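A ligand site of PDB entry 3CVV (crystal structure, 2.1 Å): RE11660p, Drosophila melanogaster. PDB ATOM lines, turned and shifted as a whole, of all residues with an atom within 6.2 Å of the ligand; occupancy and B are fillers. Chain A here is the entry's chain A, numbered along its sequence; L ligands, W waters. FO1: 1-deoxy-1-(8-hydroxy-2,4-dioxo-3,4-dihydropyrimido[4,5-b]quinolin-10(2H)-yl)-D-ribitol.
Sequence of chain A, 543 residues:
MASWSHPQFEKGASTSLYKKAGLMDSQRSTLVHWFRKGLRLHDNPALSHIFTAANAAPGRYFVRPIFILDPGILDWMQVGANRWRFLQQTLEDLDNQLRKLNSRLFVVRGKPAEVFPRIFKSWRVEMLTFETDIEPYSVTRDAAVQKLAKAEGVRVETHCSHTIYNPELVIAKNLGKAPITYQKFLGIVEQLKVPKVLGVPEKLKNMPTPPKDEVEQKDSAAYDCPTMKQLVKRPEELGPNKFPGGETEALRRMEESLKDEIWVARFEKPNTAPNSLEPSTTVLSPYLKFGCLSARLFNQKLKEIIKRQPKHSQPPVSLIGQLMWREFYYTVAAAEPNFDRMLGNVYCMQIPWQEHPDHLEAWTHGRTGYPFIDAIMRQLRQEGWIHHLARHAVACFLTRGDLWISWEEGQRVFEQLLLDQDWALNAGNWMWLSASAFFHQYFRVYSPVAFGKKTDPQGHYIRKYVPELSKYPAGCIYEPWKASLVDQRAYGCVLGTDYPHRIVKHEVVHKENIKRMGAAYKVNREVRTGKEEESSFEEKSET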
ATOM      1  N   TRP A  34      27.085 -10.757 -10.398  1.00  0.00           N
ATOM      2  CA  TRP A  34      26.801  -9.848 -11.481  1.00  0.00           C
ATOM      3  C   TRP A  34      28.112  -9.449 -12.159  1.00  0.00           C
ATOM      4  O   TRP A  34      28.920  -8.744 -11.579  1.00  0.00           O
ATOM      5  CB  TRP A  34      26.053  -8.624 -10.919  1.00  0.00           C
ATOM      6  CG  TRP A  34      25.707  -7.601 -11.920  1.00  0.00           C
ATOM      7  CD1 TRP A  34      25.591  -7.775 -13.272  1.00  0.00           C
ATOM      8  CD2 TRP A  34      25.381  -6.231 -11.661  1.00  0.00           C
ATOM      9  NE1 TRP A  34      25.248  -6.595 -13.870  1.00  0.00           N
ATOM     10  CE2 TRP A  34      25.102  -5.637 -12.905  1.00  0.00           C
ATOM     11  CE3 TRP A  34      25.317  -5.449 -10.507  1.00  0.00           C
ATOM     12  CZ2 TRP A  34      24.760  -4.284 -13.029  1.00  0.00           C
ATOM     13  CZ3 TRP A  34      24.959  -4.110 -10.625  1.00  0.00           C
ATOM     14  CH2 TRP A  34      24.691  -3.542 -11.882  1.00  0.00           C
ATOM     15  N   PHE A  35      28.303  -9.946 -13.386  1.00  0.00           N
ATOM     16  CA  PHE A  35      29.449  -9.595 -14.237  1.00  0.00           C
ATOM     17  C   PHE A  35      29.190  -8.239 -14.923  1.00  0.00           C
ATOM     18  O   PHE A  35      28.130  -8.022 -15.479  1.00  0.00           O
ATOM     19  CB  PHE A  35      29.653 -10.625 -15.354  1.00  0.00           C
ATOM     20  CG  PHE A  35      30.106 -11.978 -14.891  1.00  0.00           C
ATOM     21  CD1 PHE A  35      31.427 -12.195 -14.568  1.00  0.00           C
ATOM     22  CD2 PHE A  35      29.225 -13.044 -14.822  1.00  0.00           C
ATOM     23  CE1 PHE A  35      31.875 -13.445 -14.162  1.00  0.00           C
ATOM     24  CE2 PHE A  35      29.648 -14.288 -14.403  1.00  0.00           C
ATOM     25  CZ  PHE A  35      30.997 -14.495 -14.079  1.00  0.00           C
ATOM     26  N   ARG A  36      30.187  -7.361 -14.921  1.00  0.00           N
ATOM     27  CA  ARG A  36      30.131  -6.117 -15.730  1.00  0.00           C
ATOM     28  C   ARG A  36      31.509  -5.995 -16.389  1.00  0.00           C
ATOM     29  O   ARG A  36      31.641  -6.158 -17.613  1.00  0.00           O
ATOM     30  CB  ARG A  36      29.782  -4.878 -14.891  1.00  0.00           C
ATOM     31  CG  ARG A  36      28.591  -5.024 -13.937  1.00  0.00           C
ATOM     32  CD  ARG A  36      28.998  -5.602 -12.580  1.00  0.00           C
ATOM     33  NE  ARG A  36      29.876  -4.661 -11.876  1.00  0.00           N
ATOM     34  CZ  ARG A  36      29.451  -3.579 -11.239  1.00  0.00           C
ATOM     35  NH1 ARG A  36      28.161  -3.308 -11.150  1.00  0.00           N
ATOM     36  NH2 ARG A  36      30.334  -2.792 -10.662  1.00  0.00           N
ATOM     37  N   LYS A  37      32.522  -5.728 -15.562  1.00  0.00           N
ATOM     38  CA  LYS A  37      33.887  -6.128 -15.887  1.00  0.00           C
ATOM     39  C   LYS A  37      34.087  -7.453 -15.140  1.00  0.00           C
ATOM     40  O   LYS A  37      33.108  -8.171 -14.852  1.00  0.00           O
ATOM     41  CB  LYS A  37      34.906  -5.039 -15.480  1.00  0.00           C
ATOM     42  CG  LYS A  37      34.636  -3.663 -16.104  1.00  0.00           C
ATOM     43  CD  LYS A  37      35.599  -2.610 -15.587  1.00  0.00           C
ATOM     44  CE  LYS A  37      35.315  -1.237 -16.140  1.00  0.00           C
ATOM     45  NZ  LYS A  37      36.344  -0.228 -15.711  1.00  0.00           N
ATOM     46  N   LEU A  39      35.306 -10.126 -16.243  1.00  0.00           N
ATOM     47  CA  LEU A  39      34.731 -11.126 -17.135  1.00  0.00           C
ATOM     48  C   LEU A  39      35.589 -12.410 -17.300  1.00  0.00           C
ATOM     49  O   LEU A  39      36.062 -12.715 -18.385  1.00  0.00           O
ATOM     50  CB  LEU A  39      34.326 -10.525 -18.499  1.00  0.00           C
ATOM     51  CG  LEU A  39      33.254  -9.438 -18.514  1.00  0.00           C
ATOM     52  CD1 LEU A  39      33.075  -8.860 -19.872  1.00  0.00           C
ATOM     53  CD2 LEU A  39      31.949  -9.891 -17.955  1.00  0.00           C
ATOM     54  N   PHE A  67      25.126 -11.480 -16.652  1.00  0.00           N
ATOM     55  CA  PHE A  67      25.606 -10.277 -17.304  1.00  0.00           C
ATOM     56  C   PHE A  67      24.353  -9.557 -17.816  1.00  0.00           C
ATOM     57  O   PHE A  67      23.510 -10.163 -18.477  1.00  0.00           O
ATOM     58  CB  PHE A  67      26.565 -10.602 -18.445  1.00  0.00           C
ATOM     59  CG  PHE A  67      27.143  -9.368 -19.127  1.00  0.00           C
ATOM     60  CD1 PHE A  67      28.285  -8.761 -18.626  1.00  0.00           C
ATOM     61  CD2 PHE A  67      26.560  -8.863 -20.273  1.00  0.00           C
ATOM     62  CE1 PHE A  67      28.840  -7.642 -19.237  1.00  0.00           C
ATOM     63  CE2 PHE A  67      27.111  -7.730 -20.913  1.00  0.00           C
ATOM     64  CZ  PHE A  67      28.249  -7.140 -20.399  1.00  0.00           C
ATOM     65  N   ILE A  68      24.233  -8.279 -17.496  1.00  0.00           N
ATOM     66  CA  ILE A  68      23.101  -7.494 -17.945  1.00  0.00           C
ATOM     67  C   ILE A  68      23.511  -6.685 -19.165  1.00  0.00           C
ATOM     68  O   ILE A  68      24.320  -5.757 -19.060  1.00  0.00           O
ATOM     69  CB  ILE A  68      22.603  -6.566 -16.830  1.00  0.00           C
ATOM     70  CG1 ILE A  68      22.188  -7.393 -15.610  1.00  0.00           C
ATOM     71  CG2 ILE A  68      21.461  -5.689 -17.372  1.00  0.00           C
ATOM     72  CD1 ILE A  68      21.675  -6.568 -14.432  1.00  0.00           C
ATOM     73  N   LEU A  69      22.965  -7.049 -20.320  1.00  0.00           N
ATOM     74  CA  LEU A  69      23.239  -6.355 -21.562  1.00  0.00           C
ATOM     75  C   LEU A  69      22.353  -5.117 -21.539  1.00  0.00           C
ATOM     76  O   LEU A  69      21.142  -5.188 -21.755  1.00  0.00           O
ATOM     77  CB  LEU A  69      22.943  -7.259 -22.743  1.00  0.00           C
ATOM     78  CG  LEU A  69      23.414  -6.819 -24.135  1.00  0.00           C
ATOM     79  CD1 LEU A  69      24.924  -6.828 -24.248  1.00  0.00           C
ATOM     80  CD2 LEU A  69      22.780  -7.756 -25.200  1.00  0.00           C
ATOM     81  N   ASP A  70      23.007  -3.987 -21.273  1.00  0.00           N
ATOM     82  CA  ASP A  70      22.417  -2.777 -20.745  1.00  0.00           C
ATOM     83  C   ASP A  70      22.369  -1.729 -21.843  1.00  0.00           C
ATOM     84  O   ASP A  70      23.401  -1.182 -22.234  1.00  0.00           O
ATOM     85  CB  ASP A  70      23.293  -2.296 -19.572  1.00  0.00           C
ATOM     86  CG  ASP A  70      22.832  -0.987 -18.966  1.00  0.00           C
ATOM     87  OD1 ASP A  70      21.781  -0.435 -19.375  1.00  0.00           O
ATOM     88  OD2 ASP A  70      23.547  -0.501 -18.043  1.00  0.00           O
ATOM     89  N   PRO A  71      21.166  -1.408 -22.330  1.00  0.00           N
ATOM     90  CA  PRO A  71      20.999  -0.367 -23.357  1.00  0.00           C
ATOM     91  C   PRO A  71      21.504   1.004 -22.924  1.00  0.00           C
ATOM     92  O   PRO A  71      21.812   1.829 -23.767  1.00  0.00           O
ATOM     93  CB  PRO A  71      19.486  -0.331 -23.591  1.00  0.00           C
ATOM     94  CG  PRO A  71      18.954  -1.603 -23.055  1.00  0.00           C
ATOM     95  CD  PRO A  71      19.872  -1.999 -21.940  1.00  0.00           C
ATOM     96  N   ILE A  73      24.337   1.813 -21.671  1.00  0.00           N
ATOM     97  CA  ILE A  73      25.749   1.948 -22.038  1.00  0.00           C
ATOM     98  C   ILE A  73      25.930   2.818 -23.271  1.00  0.00           C
ATOM     99  O   ILE A  73      26.892   3.581 -23.362  1.00  0.00           O
ATOM    100  CB  ILE A  73      26.380   0.517 -22.308  1.00  0.00           C
ATOM    101  CG1 ILE A  73      26.634  -0.214 -20.987  1.00  0.00           C
ATOM    102  CG2 ILE A  73      27.674   0.625 -23.093  1.00  0.00           C
ATOM    103  CD1 ILE A  73      27.798   0.350 -20.160  1.00  0.00           C
ATOM    104  N   TRP A  76      26.115   6.547 -23.030  1.00  0.00           N
ATOM    105  CA  TRP A  76      27.354   7.035 -22.431  1.00  0.00           C
ATOM    106  C   TRP A  76      28.609   6.844 -23.280  1.00  0.00           C
ATOM    107  O   TRP A  76      29.512   7.685 -23.269  1.00  0.00           O
ATOM    108  CB  TRP A  76      27.565   6.279 -21.134  1.00  0.00           C
ATOM    109  CG  TRP A  76      28.685   6.794 -20.323  1.00  0.00           C
ATOM    110  CD1 TRP A  76      28.904   8.080 -19.962  1.00  0.00           C
ATOM    111  CD2 TRP A  76      29.729   6.017 -19.715  1.00  0.00           C
ATOM    112  NE1 TRP A  76      30.033   8.171 -19.177  1.00  0.00           N
ATOM    113  CE2 TRP A  76      30.561   6.916 -19.021  1.00  0.00           C
ATOM    114  CE3 TRP A  76      30.048   4.659 -19.713  1.00  0.00           C
ATOM    115  CZ2 TRP A  76      31.685   6.493 -18.326  1.00  0.00           C
ATOM    116  CZ3 TRP A  76      31.170   4.242 -19.025  1.00  0.00           C
ATOM    117  CH2 TRP A  76      31.970   5.167 -18.339  1.00  0.00           C
ATOM    118  N   MET A  77      28.651   5.737 -24.017  1.00  0.00           N
ATOM    119  CA  MET A  77      29.868   5.232 -24.612  1.00  0.00           C
ATOM    120  C   MET A  77      29.566   4.920 -26.086  1.00  0.00           C
ATOM    121  O   MET A  77      28.554   4.309 -26.381  1.00  0.00           O
ATOM    122  CB  MET A  77      30.209   3.933 -23.872  1.00  0.00           C
ATOM    123  CG  MET A  77      31.652   3.529 -23.824  1.00  0.00           C
ATOM    124  SD  MET A  77      31.790   1.800 -23.327  1.00  0.00           S
ATOM    125  CE  MET A  77      31.070   1.868 -21.690  1.00  0.00           C
ATOM    126  N   VAL A  79      30.674   2.503 -29.024  1.00  0.00           N
ATOM    127  CA  VAL A  79      31.267   1.169 -29.098  1.00  0.00           C
ATOM    128  C   VAL A  79      31.282   0.739 -30.568  1.00  0.00           C
ATOM    129  O   VAL A  79      30.234   0.615 -31.200  1.00  0.00           O
ATOM    130  CB  VAL A  79      30.451   0.157 -28.240  1.00  0.00           C
ATOM    131  CG1 VAL A  79      31.144  -1.202 -28.173  1.00  0.00           C
ATOM    132  CG2 VAL A  79      30.194   0.710 -26.805  1.00  0.00           C
ATOM    133  N   ARG A  83      34.885  -3.951 -31.060  1.00  0.00           N
ATOM    134  CA  ARG A  83      34.730  -4.164 -29.616  1.00  0.00           C
ATOM    135  C   ARG A  83      33.445  -4.935 -29.267  1.00  0.00           C
ATOM    136  O   ARG A  83      33.460  -5.742 -28.342  1.00  0.00           O
ATOM    137  CB  ARG A  83      34.837  -2.873 -28.816  1.00  0.00           C
ATOM    138  CG  ARG A  83      34.834  -3.123 -27.299  1.00  0.00           C
ATOM    139  CD  ARG A  83      35.532  -2.039 -26.507  1.00  0.00           C
ATOM    140  NE  ARG A  83      34.670  -0.910 -26.135  1.00  0.00           N
ATOM    141  CZ  ARG A  83      34.471   0.171 -26.881  1.00  0.00           C
ATOM    142  NH1 ARG A  83      35.035   0.326 -28.075  1.00  0.00           N
ATOM    143  NH2 ARG A  83      33.679   1.116 -26.434  1.00  0.00           N
ATOM    144  N   TRP A  84      32.346  -4.708 -29.981  1.00  0.00           N
ATOM    145  CA  TRP A  84      31.150  -5.563 -29.846  1.00  0.00           C
ATOM    146  C   TRP A  84      31.453  -7.010 -30.099  1.00  0.00           C
ATOM    147  O   TRP A  84      30.973  -7.876 -29.365  1.00  0.00           O
ATOM    148  CB  TRP A  84      30.026  -5.132 -30.797  1.00  0.00           C
ATOM    149  CG  TRP A  84      29.288  -3.951 -30.305  1.00  0.00           C
ATOM    150  CD1 TRP A  84      29.158  -2.763 -30.934  1.00  0.00           C
ATOM    151  CD2 TRP A  84      28.571  -3.839 -29.071  1.00  0.00           C
ATOM    152  NE1 TRP A  84      28.416  -1.904 -30.179  1.00  0.00           N
ATOM    153  CE2 TRP A  84      28.047  -2.539 -29.021  1.00  0.00           C
ATOM    154  CE3 TRP A  84      28.332  -4.705 -27.997  1.00  0.00           C
ATOM    155  CZ2 TRP A  84      27.291  -2.089 -27.954  1.00  0.00           C
ATOM    156  CZ3 TRP A  84      27.590  -4.265 -26.929  1.00  0.00           C
ATOM    157  CH2 TRP A  84      27.086  -2.958 -26.906  1.00  0.00           C
ATOM    158  N   LEU A  87      33.326  -8.422 -27.141  1.00  0.00           N
ATOM    159  CA  LEU A  87      32.413  -8.712 -26.058  1.00  0.00           C
ATOM    160  C   LEU A  87      31.587  -9.979 -26.325  1.00  0.00           C
ATOM    161  O   LEU A  87      31.388 -10.788 -25.419  1.00  0.00           O
ATOM    162  CB  LEU A  87      31.474  -7.535 -25.811  1.00  0.00           C
ATOM    163  CG  LEU A  87      30.478  -7.734 -24.662  1.00  0.00           C
ATOM    164  CD1 LEU A  87      31.231  -8.068 -23.358  1.00  0.00           C
ATOM    165  CD2 LEU A  87      29.604  -6.525 -24.476  1.00  0.00           C
ATOM    166  N   PRO A 112      19.748  -2.286 -15.749  1.00  0.00           N
ATOM    167  CA  PRO A 112      19.824  -2.744 -14.361  1.00  0.00           C
ATOM    168  C   PRO A 112      18.708  -2.236 -13.463  1.00  0.00           C
ATOM    169  O   PRO A 112      18.118  -3.039 -12.749  1.00  0.00           O
ATOM    170  CB  PRO A 112      21.176  -2.198 -13.898  1.00  0.00           C
ATOM    171  CG  PRO A 112      22.013  -2.262 -15.126  1.00  0.00           C
ATOM    172  CD  PRO A 112      21.071  -1.861 -16.243  1.00  0.00           C
ATOM    173  N   ASP A 133      33.828  -0.906  -9.483  1.00  0.00           N
ATOM    174  CA  ASP A 133      34.409  -0.085 -10.537  1.00  0.00           C
ATOM    175  C   ASP A 133      34.196   1.393 -10.188  1.00  0.00           C
ATOM    176  O   ASP A 133      33.228   1.748  -9.500  1.00  0.00           O
ATOM    177  CB  ASP A 133      33.774  -0.421 -11.875  1.00  0.00           C
ATOM    178  CG  ASP A 133      34.501   0.212 -13.048  1.00  0.00           C
ATOM    179  OD1 ASP A 133      35.754   0.239 -13.077  1.00  0.00           O
ATOM    180  OD2 ASP A 133      33.784   0.670 -13.961  1.00  0.00           O
ATOM    181  N   GLU A 135      34.141   4.098 -12.469  1.00  0.00           N
ATOM    182  CA  GLU A 135      33.673   4.955 -13.568  1.00  0.00           C
ATOM    183  C   GLU A 135      32.353   5.604 -13.143  1.00  0.00           C
ATOM    184  O   GLU A 135      31.591   5.008 -12.382  1.00  0.00           O
ATOM    185  CB  GLU A 135      33.480   4.158 -14.851  1.00  0.00           C
ATOM    186  CG  GLU A 135      34.725   3.455 -15.302  1.00  0.00           C
ATOM    187  CD  GLU A 135      34.564   2.656 -16.568  1.00  0.00           C
ATOM    188  OE1 GLU A 135      33.462   2.604 -17.146  1.00  0.00           O
ATOM    189  OE2 GLU A 135      35.598   2.098 -16.989  1.00  0.00           O
ATOM    190  N   PRO A 136      32.082   6.831 -13.624  1.00  0.00           N
ATOM    191  CA  PRO A 136      30.819   7.509 -13.272  1.00  0.00           C
ATOM    192  C   PRO A 136      29.565   6.702 -13.601  1.00  0.00           C
ATOM    193  O   PRO A 136      28.629   6.698 -12.832  1.00  0.00           O
ATOM    194  CB  PRO A 136      30.849   8.809 -14.084  1.00  0.00           C
ATOM    195  CG  PRO A 136      32.035   8.742 -14.966  1.00  0.00           C
ATOM    196  CD  PRO A 136      32.942   7.655 -14.485  1.00  0.00           C
ATOM    197  N   TYR A 137      29.555   6.020 -14.739  1.00  0.00           N
ATOM    198  CA  TYR A 137      28.440   5.161 -15.074  1.00  0.00           C
ATOM    199  C   TYR A 137      28.229   4.139 -13.970  1.00  0.00           C
ATOM    200  O   TYR A 137      27.125   3.994 -13.443  1.00  0.00           O
ATOM    201  CB  TYR A 137      28.693   4.442 -16.409  1.00  0.00           C
ATOM    202  CG  TYR A 137      27.486   3.731 -16.956  1.00  0.00           C
ATOM    203  CD1 TYR A 137      26.592   4.403 -17.774  1.00  0.00           C
ATOM    204  CD2 TYR A 137      27.227   2.402 -16.653  1.00  0.00           C
ATOM    205  CE1 TYR A 137      25.485   3.764 -18.286  1.00  0.00           C
ATOM    206  CE2 TYR A 137      26.114   1.746 -17.151  1.00  0.00           C
ATOM    207  CZ  TYR A 137      25.243   2.442 -17.968  1.00  0.00           C
ATOM    208  OH  TYR A 137      24.131   1.816 -18.495  1.00  0.00           O
ATOM    209  N   SER A 138      29.317   3.472 -13.594  1.00  0.00           N
ATOM    210  CA  SER A 138      29.259   2.432 -12.594  1.00  0.00           C
ATOM    211  C   SER A 138      28.872   2.969 -11.216  1.00  0.00           C
ATOM    212  O   SER A 138      28.128   2.303 -10.483  1.00  0.00           O
ATOM    213  CB  SER A 138      30.609   1.717 -12.494  1.00  0.00           C
ATOM    214  OG  SER A 138      30.459   0.559 -11.697  1.00  0.00           O
ATOM    215  N   VAL A 139      29.376   4.140 -10.867  1.00  0.00           N
ATOM    216  CA  VAL A 139      29.066   4.737  -9.570  1.00  0.00           C
ATOM    217  C   VAL A 139      27.566   4.963  -9.442  1.00  0.00           C
ATOM    218  O   VAL A 139      26.970   4.615  -8.426  1.00  0.00           O
ATOM    219  CB  VAL A 139      29.839   6.058  -9.334  1.00  0.00           C
ATOM    220  CG1 VAL A 139      29.278   6.810  -8.136  1.00  0.00           C
ATOM    221  CG2 VAL A 139      31.328   5.790  -9.136  1.00  0.00           C
ATOM    222  N   ARG A 141      25.040   3.659 -11.306  1.00  0.00           N
ATOM    223  CA  ARG A 141      24.380   2.364 -11.444  1.00  0.00           C
ATOM    224  C   ARG A 141      24.381   1.568 -10.158  1.00  0.00           C
ATOM    225  O   ARG A 141      23.331   1.138  -9.684  1.00  0.00           O
ATOM    226  CB  ARG A 141      25.072   1.567 -12.542  1.00  0.00           C
ATOM    227  CG  ARG A 141      24.578   0.161 -12.719  1.00  0.00           C
ATOM    228  CD  ARG A 141      25.432  -0.538 -13.737  1.00  0.00           C
ATOM    229  NE  ARG A 141      26.819  -0.695 -13.284  1.00  0.00           N
ATOM    230  CZ  ARG A 141      27.823  -1.076 -14.061  1.00  0.00           C
ATOM    231  NH1 ARG A 141      27.612  -1.347 -15.333  1.00  0.00           N
ATOM    232  NH2 ARG A 141      29.042  -1.170 -13.567  1.00  0.00           N
ATOM    233  N   LYS A 289      41.133  -4.747 -19.856  1.00  0.00           N
ATOM    234  CA  LYS A 289      40.023  -3.805 -19.880  1.00  0.00           C
ATOM    235  C   LYS A 289      38.686  -4.468 -19.556  1.00  0.00           C
ATOM    236  O   LYS A 289      37.909  -3.928 -18.787  1.00  0.00           O
ATOM    237  CB  LYS A 289      39.968  -3.056 -21.218  1.00  0.00           C
ATOM    238  CG  LYS A 289      38.674  -2.293 -21.499  1.00  0.00           C
ATOM    239  CD  LYS A 289      37.655  -3.147 -22.261  1.00  0.00           C
ATOM    240  CE  LYS A 289      36.620  -2.300 -22.960  1.00  0.00           C
ATOM    241  NZ  LYS A 289      35.823  -1.519 -22.010  1.00  0.00           N
ATOM    242  N   PHE A 290      38.420  -5.634 -20.153  1.00  0.00           N
ATOM    243  CA  PHE A 290      37.157  -6.338 -19.916  1.00  0.00           C
ATOM    244  C   PHE A 290      37.174  -7.220 -18.672  1.00  0.00           C
ATOM    245  O   PHE A 290      36.122  -7.697 -18.226  1.00  0.00           O
ATOM    246  CB  PHE A 290      36.778  -7.192 -21.124  1.00  0.00           C
ATOM    247  CG  PHE A 290      35.992  -6.461 -22.184  1.00  0.00           C
ATOM    248  CD1 PHE A 290      36.551  -6.233 -23.435  1.00  0.00           C
ATOM    249  CD2 PHE A 290      34.690  -6.069 -21.968  1.00  0.00           C
ATOM    250  CE1 PHE A 290      35.823  -5.599 -24.435  1.00  0.00           C
ATOM    251  CE2 PHE A 290      33.952  -5.439 -22.954  1.00  0.00           C
ATOM    252  CZ  PHE A 290      34.520  -5.207 -24.206  1.00  0.00           C
ATOM    253  N   LEU A 419      39.618  -1.787 -28.906  1.00  0.00           N
ATOM    254  CA  LEU A 419      39.126  -2.970 -28.192  1.00  0.00           C
ATOM    255  C   LEU A 419      39.353  -2.801 -26.686  1.00  0.00           C
ATOM    256  O   LEU A 419      38.571  -3.298 -25.885  1.00  0.00           O
ATOM    257  CB  LEU A 419      39.863  -4.234 -28.648  1.00  0.00           C
ATOM    258  CG  LEU A 419      39.783  -4.671 -30.110  1.00  0.00           C
ATOM    259  CD1 LEU A 419      40.747  -5.831 -30.362  1.00  0.00           C
ATOM    260  CD2 LEU A 419      38.392  -5.054 -30.483  1.00  0.00           C
ATOM    261  N   GLN A 421      39.311   0.091 -25.030  1.00  0.00           N
ATOM    262  CA  GLN A 421      38.665   1.316 -24.554  1.00  0.00           C
ATOM    263  C   GLN A 421      38.433   1.286 -23.059  1.00  0.00           C
ATOM    264  O   GLN A 421      37.644   0.497 -22.561  1.00  0.00           O
ATOM    265  CB  GLN A 421      37.333   1.533 -25.274  1.00  0.00           C
ATOM    266  CG  GLN A 421      36.640   2.865 -24.937  1.00  0.00           C
ATOM    267  CD  GLN A 421      35.779   2.851 -23.689  1.00  0.00           C
ATOM    268  OE1 GLN A 421      35.792   3.815 -22.906  1.00  0.00           O
ATOM    269  NE2 GLN A 421      35.011   1.780 -23.494  1.00  0.00           N
HETATM  270  N1  FO1 L   1      28.628  -3.592 -19.026  1.00  0.00           N
HETATM  271  C1  FO1 L   1      27.386  -4.035 -18.726  1.00  0.00           C
HETATM  272  O1  FO1 L   1      27.047  -4.237 -17.533  1.00  0.00           O
HETATM  273  N2  FO1 L   1      26.474  -4.265 -19.689  1.00  0.00           N
HETATM  274  C2  FO1 L   1      26.754  -4.089 -20.985  1.00  0.00           C
HETATM  275  O2  FO1 L   1      25.876  -4.311 -21.855  1.00  0.00           O
HETATM  276  C3  FO1 L   1      28.109  -3.596 -21.357  1.00  0.00           C
HETATM  277  C4  FO1 L   1      28.462  -3.383 -22.684  1.00  0.00           C
HETATM  278  C5  FO1 L   1      29.737  -2.913 -23.011  1.00  0.00           C
HETATM  279  C6  FO1 L   1      30.112  -2.676 -24.322  1.00  0.00           C
HETATM  280  C7  FO1 L   1      31.401  -2.198 -24.564  1.00  0.00           C
HETATM  281  C9  FO1 L   1      32.265  -1.998 -23.475  1.00  0.00           C
HETATM  282  O10 FO1 L   1      33.506  -1.532 -23.740  1.00  0.00           O
HETATM  283  C11 FO1 L   1      31.909  -2.221 -22.226  1.00  0.00           C
HETATM  284  C12 FO1 L   1      30.730  -2.685 -21.922  1.00  0.00           C
HETATM  285  N3  FO1 L   1      30.317  -2.859 -20.571  1.00  0.00           N
HETATM  286  C13 FO1 L   1      29.024  -3.384 -20.315  1.00  0.00           C
HETATM  287  C14 FO1 L   1      31.356  -3.140 -19.555  1.00  0.00           C
HETATM  288  C15 FO1 L   1      31.539  -1.783 -18.843  1.00  0.00           C
HETATM  289  O3  FO1 L   1      32.883  -1.343 -19.038  1.00  0.00           O
HETATM  290  C16 FO1 L   1      31.186  -1.831 -17.354  1.00  0.00           C
HETATM  291  O4  FO1 L   1      29.782  -2.014 -17.170  1.00  0.00           O
HETATM  292  C17 FO1 L   1      31.551  -0.560 -16.595  1.00  0.00           C
HETATM  293  O5  FO1 L   1      31.517  -0.879 -15.200  1.00  0.00           O
HETATM  294  C18 FO1 L   1      30.600   0.607 -16.838  1.00  0.00           C
HETATM  295  O6  FO1 L   1      31.034   1.701 -16.025  1.00  0.00           O
HETATM  296  O   HOH W   1      26.264  -6.588 -16.539  1.00  0.00           O
HETATM  297  O   HOH W   2      24.892  -2.751 -23.985  1.00  0.00           O
HETATM  298  O   HOH W   3      35.004  -2.799 -19.734  1.00  0.00           O
HETATM  299  O   HOH W   4      25.193  -2.492 -16.547  1.00  0.00           O
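O2 of the ligand is in hydrogen-bond range of N of Asp 70, at 2.9 Å.
An oxygen (O5) of the ligand lies within hydrogen-bond range of the side-chain carboxylate (OD2) of Asp 133 (3.0 Å).
The guanidinium group of Arg 83 sits at hydrogen-bond distance from an oxygen (O10) of the ligand, at 2.7 Å.
An oxygen (O4) of the ligand is in hydrogen-bond range of the guanidinium group (NH1) of Arg 141 (2.9 Å).
The side-chain sulfur of Met 77 lies within hydrogen-bond range of an oxygen (O10) of the ligand (3.8 Å).
The side-chain carboxylate (OE1) of Glu 135 lies within hydrogen-bond range of an oxygen (O6) of the ligand (2.8 Å).
A nitrogen (N2) of the ligand lies within hydrogen-bond range of the backbone carbonyl oxygen (O) of Ile 68, at 2.7 Å.
O10 of the ligand is in hydrogen-bond range of NZ of Lys 289, 2.9 Å away.
N of Ser 138 is in hydrogen-bond range of O6 of the ligand, at 3.5 Å.
OD1 of Asp 133 lies within salt-bridge range of NZ of Lys 37 (2.7 Å).
The backbone carbonyl oxygen of Val 79 lies within hydrogen-bond range of the indole nitrogen of Trp 84, 3.3 Å away.
OG of Ser 138 lies within hydrogen-bond range of NH2 of Arg 141.
OE2 of Glu 135 lies within salt-bridge range of NZ of Lys 37.
The side-chain amide nitrogen (NE2) of Gln 421 sits at hydrogen-bond distance from the side-chain sulfur (SD) of Met 77 (3.2 Å).
The backbone carbonyl oxygen (O) of Gln 421 lies within hydrogen-bond range of the side-chain amino group (NZ) of Lys 289, 2.8 Å away.
The backbone NH of Leu 39 is in hydrogen-bond range of the backbone carbonyl oxygen of Phe 290.
OH of Tyr 137 is in hydrogen-bond range of N of Ile 73, 3.2 Å away.
Residues that only touch the ligand: Arg 36 (3.6 Å), Lys 37 (3.8 Å), Phe 67 (3.4 Å), Leu 69 (3.3 Å), Ile 73 (3.7 Å), Trp 76 (3.9 Å), Val 79 (3.8 Å), Trp 84 (3.96 Å), Leu 87 (3.8 Å), Tyr 137 (3.6 Å), Phe 290 (3.8 Å) and Gln 421 (3.6 Å).
Hydrophobic or aromatic side chains within 4 Å of the ligand: Phe 67, Leu 69, Ile 73, Trp 76, Met 77, Val 79, Trp 84, Leu 87, Tyr 137 and Phe 290.
Water W3 lies within hydrogen-bond range of O3 of the ligand (2.7 Å) and NZ of Lys 289 (2.7 Å).
Water W1 lies within hydrogen-bond range of O of Phe 35, O1 of the ligand, N of Ile 68 and NE1 of Trp 34.
Water W4 lies within hydrogen-bond range of an oxygen (O1) of the ligand (2.7 Å), the guanidinium group (NH1) of Arg 141 (2.9 Å) and the side-chain carboxylate (OD2) of Asp 70 (3.0 Å).
Water W2 bridges O of Asp 70 (2.8 Å) and O2 of the ligand (2.8 Å).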
